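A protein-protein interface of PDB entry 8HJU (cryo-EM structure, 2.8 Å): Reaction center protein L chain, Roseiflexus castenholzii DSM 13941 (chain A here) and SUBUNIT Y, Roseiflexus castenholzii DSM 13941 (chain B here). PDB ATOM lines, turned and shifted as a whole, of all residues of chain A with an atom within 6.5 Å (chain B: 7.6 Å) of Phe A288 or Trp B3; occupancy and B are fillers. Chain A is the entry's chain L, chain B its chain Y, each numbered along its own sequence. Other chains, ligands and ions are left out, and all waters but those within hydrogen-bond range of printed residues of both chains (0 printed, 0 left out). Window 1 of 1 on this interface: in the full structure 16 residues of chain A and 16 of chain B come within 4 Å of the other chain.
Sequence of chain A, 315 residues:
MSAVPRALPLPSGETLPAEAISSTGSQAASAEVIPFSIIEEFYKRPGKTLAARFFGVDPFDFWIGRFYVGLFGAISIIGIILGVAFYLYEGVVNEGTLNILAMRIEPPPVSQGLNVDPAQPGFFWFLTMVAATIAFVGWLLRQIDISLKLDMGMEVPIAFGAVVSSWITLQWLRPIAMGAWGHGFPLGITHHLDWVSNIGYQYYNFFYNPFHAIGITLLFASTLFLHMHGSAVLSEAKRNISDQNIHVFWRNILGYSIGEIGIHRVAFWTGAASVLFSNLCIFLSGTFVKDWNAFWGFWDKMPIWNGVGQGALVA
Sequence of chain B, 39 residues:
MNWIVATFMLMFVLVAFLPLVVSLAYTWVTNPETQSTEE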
ATOM      1  N   PHE A 283      -1.014 -11.971  -0.510  1.00  0.00           N
ATOM      2  CA  PHE A 283      -2.050 -12.855   0.003  1.00  0.00           C
ATOM      3  C   PHE A 283      -2.340 -13.975  -0.981  1.00  0.00           C
ATOM      4  O   PHE A 283      -2.428 -15.146  -0.595  1.00  0.00           O
ATOM      5  CB  PHE A 283      -3.324 -12.078   0.317  1.00  0.00           C
ATOM      6  CG  PHE A 283      -4.422 -12.940   0.850  1.00  0.00           C
ATOM      7  CD1 PHE A 283      -4.519 -13.194   2.202  1.00  0.00           C
ATOM      8  CD2 PHE A 283      -5.336 -13.527  -0.002  1.00  0.00           C
ATOM      9  CE1 PHE A 283      -5.509 -14.000   2.691  1.00  0.00           C
ATOM     10  CE2 PHE A 283      -6.323 -14.334   0.482  1.00  0.00           C
ATOM     11  CZ  PHE A 283      -6.413 -14.571   1.828  1.00  0.00           C
ATOM     12  N   LEU A 284      -2.502 -13.640  -2.263  1.00  0.00           N
ATOM     13  CA  LEU A 284      -2.722 -14.682  -3.259  1.00  0.00           C
ATOM     14  C   LEU A 284      -1.534 -15.623  -3.336  1.00  0.00           C
ATOM     15  O   LEU A 284      -1.696 -16.827  -3.558  1.00  0.00           O
ATOM     16  CB  LEU A 284      -2.984 -14.057  -4.624  1.00  0.00           C
ATOM     17  CG  LEU A 284      -4.344 -13.411  -4.825  1.00  0.00           C
ATOM     18  CD1 LEU A 284      -4.530 -13.119  -6.284  1.00  0.00           C
ATOM     19  CD2 LEU A 284      -5.445 -14.310  -4.305  1.00  0.00           C
ATOM     20  N   SER A 285      -0.326 -15.087  -3.163  1.00  0.00           N
ATOM     21  CA  SER A 285       0.870 -15.910  -3.240  1.00  0.00           C
ATOM     22  C   SER A 285       0.856 -16.991  -2.180  1.00  0.00           C
ATOM     23  O   SER A 285       1.210 -18.140  -2.449  1.00  0.00           O
ATOM     24  CB  SER A 285       2.102 -15.031  -3.094  1.00  0.00           C
ATOM     25  OG  SER A 285       2.212 -14.139  -4.179  1.00  0.00           O
ATOM     26  N   GLY A 286       0.434 -16.653  -0.970  1.00  0.00           N
ATOM     27  CA  GLY A 286       0.312 -17.691   0.038  1.00  0.00           C
ATOM     28  C   GLY A 286      -0.728 -18.745  -0.308  1.00  0.00           C
ATOM     29  O   GLY A 286      -0.429 -19.938  -0.361  1.00  0.00           O
ATOM     30  N   THR A 287      -1.962 -18.312  -0.564  1.00  0.00           N
ATOM     31  CA  THR A 287      -3.144 -19.155  -0.431  1.00  0.00           C
ATOM     32  C   THR A 287      -3.604 -19.823  -1.719  1.00  0.00           C
ATOM     33  O   THR A 287      -3.956 -21.004  -1.696  1.00  0.00           O
ATOM     34  CB  THR A 287      -4.298 -18.330   0.133  1.00  0.00           C
ATOM     35  OG1 THR A 287      -4.553 -17.225  -0.739  1.00  0.00           O
ATOM     36  CG2 THR A 287      -3.933 -17.800   1.497  1.00  0.00           C
ATOM     37  N   PHE A 288      -3.639 -19.111  -2.838  1.00  0.00           N
ATOM     38  CA  PHE A 288      -4.240 -19.648  -4.053  1.00  0.00           C
ATOM     39  C   PHE A 288      -3.235 -20.049  -5.118  1.00  0.00           C
ATOM     40  O   PHE A 288      -3.491 -20.985  -5.871  1.00  0.00           O
ATOM     41  CB  PHE A 288      -5.219 -18.636  -4.645  1.00  0.00           C
ATOM     42  CG  PHE A 288      -6.496 -18.520  -3.873  1.00  0.00           C
ATOM     43  CD1 PHE A 288      -7.405 -19.559  -3.859  1.00  0.00           C
ATOM     44  CD2 PHE A 288      -6.783 -17.381  -3.152  1.00  0.00           C
ATOM     45  CE1 PHE A 288      -8.578 -19.456  -3.146  1.00  0.00           C
ATOM     46  CE2 PHE A 288      -7.949 -17.276  -2.436  1.00  0.00           C
ATOM     47  CZ  PHE A 288      -8.850 -18.310  -2.435  1.00  0.00           C
ATOM     48  N   VAL A 289      -2.097 -19.370  -5.204  1.00  0.00           N
ATOM     49  CA  VAL A 289      -1.100 -19.628  -6.234  1.00  0.00           C
ATOM     50  C   VAL A 289       0.175 -20.098  -5.553  1.00  0.00           C
ATOM     51  O   VAL A 289       0.742 -19.378  -4.729  1.00  0.00           O
ATOM     52  CB  VAL A 289      -0.840 -18.380  -7.089  1.00  0.00           C
ATOM     53  CG1 VAL A 289       0.146 -18.692  -8.183  1.00  0.00           C
ATOM     54  CG2 VAL A 289      -2.132 -17.869  -7.677  1.00  0.00           C
ATOM     55  N   LYS A 290       0.632 -21.299  -5.901  1.00  0.00           N
ATOM     56  CA  LYS A 290       1.882 -21.797  -5.339  1.00  0.00           C
ATOM     57  C   LYS A 290       3.070 -21.461  -6.227  1.00  0.00           C
ATOM     58  O   LYS A 290       4.190 -21.305  -5.736  1.00  0.00           O
ATOM     59  CB  LYS A 290       1.799 -23.305  -5.122  1.00  0.00           C
ATOM     60  CG  LYS A 290       0.816 -23.710  -4.060  1.00  0.00           C
ATOM     61  CD  LYS A 290       0.761 -25.213  -3.908  1.00  0.00           C
ATOM     62  CE  LYS A 290      -0.208 -25.609  -2.823  1.00  0.00           C
ATOM     63  NZ  LYS A 290      -0.281 -27.082  -2.691  1.00  0.00           N
ATOM     64  N   MET B   1     -12.507 -25.130   6.117  1.00  0.00           N
ATOM     65  CA  MET B   1     -11.874 -23.972   6.733  1.00  0.00           C
ATOM     66  C   MET B   1     -10.869 -23.331   5.792  1.00  0.00           C
ATOM     67  O   MET B   1     -10.754 -22.115   5.739  1.00  0.00           O
ATOM     68  CB  MET B   1     -11.182 -24.362   8.043  1.00  0.00           C
ATOM     69  CG  MET B   1     -12.130 -24.712   9.195  1.00  0.00           C
ATOM     70  SD  MET B   1     -13.841 -24.223   8.890  1.00  0.00           S
ATOM     71  CE  MET B   1     -13.796 -22.484   9.319  1.00  0.00           C
ATOM     72  N   ASN B   2     -10.142 -24.157   5.042  1.00  0.00           N
ATOM     73  CA  ASN B   2      -9.126 -23.623   4.145  1.00  0.00           C
ATOM     74  C   ASN B   2      -9.728 -22.614   3.177  1.00  0.00           C
ATOM     75  O   ASN B   2      -9.314 -21.453   3.143  1.00  0.00           O
ATOM     76  CB  ASN B   2      -8.437 -24.763   3.392  1.00  0.00           C
ATOM     77  CG  ASN B   2      -7.178 -24.311   2.662  1.00  0.00           C
ATOM     78  OD1 ASN B   2      -6.491 -23.392   3.103  1.00  0.00           O
ATOM     79  ND2 ASN B   2      -6.870 -24.960   1.545  1.00  0.00           N
ATOM     80  N   TRP B   3     -10.722 -23.030   2.391  1.00  0.00           N
ATOM     81  CA  TRP B   3     -11.233 -22.141   1.354  1.00  0.00           C
ATOM     82  C   TRP B   3     -12.218 -21.115   1.898  1.00  0.00           C
ATOM     83  O   TRP B   3     -12.245 -19.982   1.411  1.00  0.00           O
ATOM     84  CB  TRP B   3     -11.874 -22.946   0.226  1.00  0.00           C
ATOM     85  CG  TRP B   3     -10.920 -23.872  -0.457  1.00  0.00           C
ATOM     86  CD1 TRP B   3     -11.045 -25.221  -0.586  1.00  0.00           C
ATOM     87  CD2 TRP B   3      -9.695 -23.522  -1.110  1.00  0.00           C
ATOM     88  NE1 TRP B   3      -9.976 -25.733  -1.273  1.00  0.00           N
ATOM     89  CE2 TRP B   3      -9.131 -24.708  -1.603  1.00  0.00           C
ATOM     90  CE3 TRP B   3      -9.018 -22.318  -1.322  1.00  0.00           C
ATOM     91  CZ2 TRP B   3      -7.924 -24.730  -2.293  1.00  0.00           C
ATOM     92  CZ3 TRP B   3      -7.822 -22.344  -2.009  1.00  0.00           C
ATOM     93  CH2 TRP B   3      -7.288 -23.538  -2.486  1.00  0.00           C
ATOM     94  N   ILE B   4     -13.019 -21.466   2.902  1.00  0.00           N
ATOM     95  CA  ILE B   4     -13.931 -20.482   3.472  1.00  0.00           C
ATOM     96  C   ILE B   4     -13.147 -19.361   4.140  1.00  0.00           C
ATOM     97  O   ILE B   4     -13.368 -18.175   3.870  1.00  0.00           O
ATOM     98  CB  ILE B   4     -14.905 -21.147   4.458  1.00  0.00           C
ATOM     99  CG1 ILE B   4     -15.620 -22.319   3.804  1.00  0.00           C
ATOM    100  CG2 ILE B   4     -15.925 -20.144   4.952  1.00  0.00           C
ATOM    101  CD1 ILE B   4     -16.682 -22.920   4.675  1.00  0.00           C
ATOM    102  N   VAL B   5     -12.219 -19.722   5.027  1.00  0.00           N
ATOM    103  CA  VAL B   5     -11.429 -18.718   5.729  1.00  0.00           C
ATOM    104  C   VAL B   5     -10.546 -17.963   4.752  1.00  0.00           C
ATOM    105  O   VAL B   5     -10.364 -16.743   4.865  1.00  0.00           O
ATOM    106  CB  VAL B   5     -10.603 -19.378   6.844  1.00  0.00           C
ATOM    107  CG1 VAL B   5      -9.857 -18.331   7.625  1.00  0.00           C
ATOM    108  CG2 VAL B   5     -11.501 -20.181   7.751  1.00  0.00           C
ATOM    109  N   ALA B   6      -9.985 -18.672   3.774  1.00  0.00           N
ATOM    110  CA  ALA B   6      -9.140 -18.020   2.787  1.00  0.00           C
ATOM    111  C   ALA B   6      -9.920 -16.988   1.992  1.00  0.00           C
ATOM    112  O   ALA B   6      -9.415 -15.896   1.718  1.00  0.00           O
ATOM    113  CB  ALA B   6      -8.524 -19.056   1.854  1.00  0.00           C
ATOM    114  N   THR B   7     -11.158 -17.301   1.625  1.00  0.00           N
ATOM    115  CA  THR B   7     -11.923 -16.343   0.841  1.00  0.00           C
ATOM    116  C   THR B   7     -12.418 -15.190   1.702  1.00  0.00           C
ATOM    117  O   THR B   7     -12.536 -14.060   1.220  1.00  0.00           O
ATOM    118  CB  THR B   7     -13.076 -17.042   0.133  1.00  0.00           C
ATOM    119  OG1 THR B   7     -12.643 -18.330  -0.304  1.00  0.00           O
ATOM    120  CG2 THR B   7     -13.505 -16.236  -1.060  1.00  0.00           C
ATOM    121  N   PHE B   8     -12.678 -15.435   2.983  1.00  0.00           N
ATOM    122  CA  PHE B   8     -13.011 -14.319   3.861  1.00  0.00           C
ATOM    123  C   PHE B   8     -11.837 -13.353   3.991  1.00  0.00           C
ATOM    124  O   PHE B   8     -12.012 -12.127   3.939  1.00  0.00           O
ATOM    125  CB  PHE B   8     -13.452 -14.843   5.223  1.00  0.00           C
ATOM    126  CG  PHE B   8     -14.932 -15.038   5.337  1.00  0.00           C
ATOM    127  CD1 PHE B   8     -15.756 -13.981   5.665  1.00  0.00           C
ATOM    128  CD2 PHE B   8     -15.503 -16.274   5.113  1.00  0.00           C
ATOM    129  CE1 PHE B   8     -17.117 -14.153   5.771  1.00  0.00           C
ATOM    130  CE2 PHE B   8     -16.864 -16.453   5.217  1.00  0.00           C
ATOM    131  CZ  PHE B   8     -17.670 -15.392   5.547  1.00  0.00           C
ATOM    132  N   MET B   9     -10.624 -13.880   4.122  1.00  0.00           N
ATOM    133  CA  MET B   9      -9.471 -12.990   4.187  1.00  0.00           C
ATOM    134  C   MET B   9      -9.214 -12.300   2.847  1.00  0.00           C
ATOM    135  O   MET B   9      -8.807 -11.130   2.811  1.00  0.00           O
ATOM    136  CB  MET B   9      -8.248 -13.771   4.649  1.00  0.00           C
ATOM    137  CG  MET B   9      -8.498 -14.631   5.875  1.00  0.00           C
ATOM    138  SD  MET B   9      -9.405 -13.797   7.184  1.00  0.00           S
ATOM    139  CE  MET B   9      -8.080 -13.408   8.308  1.00  0.00           C
ATOM    140  N   LEU B  10      -9.452 -13.000   1.738  1.00  0.00           N
ATOM    141  CA  LEU B  10      -9.377 -12.362   0.430  1.00  0.00           C
ATOM    142  C   LEU B  10     -10.323 -11.176   0.347  1.00  0.00           C
ATOM    143  O   LEU B  10      -9.970 -10.106  -0.173  1.00  0.00           O
ATOM    144  CB  LEU B  10      -9.720 -13.379  -0.654  1.00  0.00           C
ATOM    145  CG  LEU B  10      -9.776 -12.929  -2.107  1.00  0.00           C
ATOM    146  CD1 LEU B  10      -8.410 -12.451  -2.543  1.00  0.00           C
ATOM    147  CD2 LEU B  10     -10.258 -14.054  -2.982  1.00  0.00           C
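Printed residues of chain B that touch a printed residue of chain A: Trp B3, Ala B6, Met B9 and Leu B10.
Of the 8 printed residues of chain A, 3 touch a printed residue of chain B.
Hydrophobic or aromatic side chains of chain A that line the printed part of chain B: Phe A283, Leu A284 and Phe A288.
Among the printed residues, no Asp or Glu carboxylate lies within 4 Å of a Lys or Arg side-chain nitrogen of the other chain.
Of the printed residues of chain B, Phe A288 touches Trp B3 (3.2 Å).
Of chain A, only Phe A288 comes within 4 Å of Trp B3.
Of the printed residues of chain A, Leu B10 touches Phe A283 (3.4 Å) and Leu A284 (3.9 Å).
Of the printed residues of chain B, Leu A284 touches Leu B10.
Of the printed residues of chain A, Met B9 touches Phe A283 (3.4 Å).
Printed residues of chain A within 4 Å of Ala B6: Phe A283 (3.3 Å).
The nearest printed residue of chain B that does not touch Phe A288 is Leu B10 (4.001 Å).
Among the printed residues, pairs that only touch across the chains: Phe A283 with Ala B6, Phe A283 with Met B9, Phe A283 with Leu B10, Leu A284 with Leu B10 and Phe A288 with Trp B3.
The backbone carbonyl oxygen (O) of Phe A283 lies within hydrogen-bond range of the side-chain hydroxyl (OG1) of Thr A287 (3.0 Å).
The side-chain hydroxyl of Thr B7 sits at hydrogen-bond distance from the backbone carbonyl oxygen of Trp B3, at 2.4 Å.
N of Val A289 is in hydrogen-bond range of O of Leu A284, 3.1 Å away.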
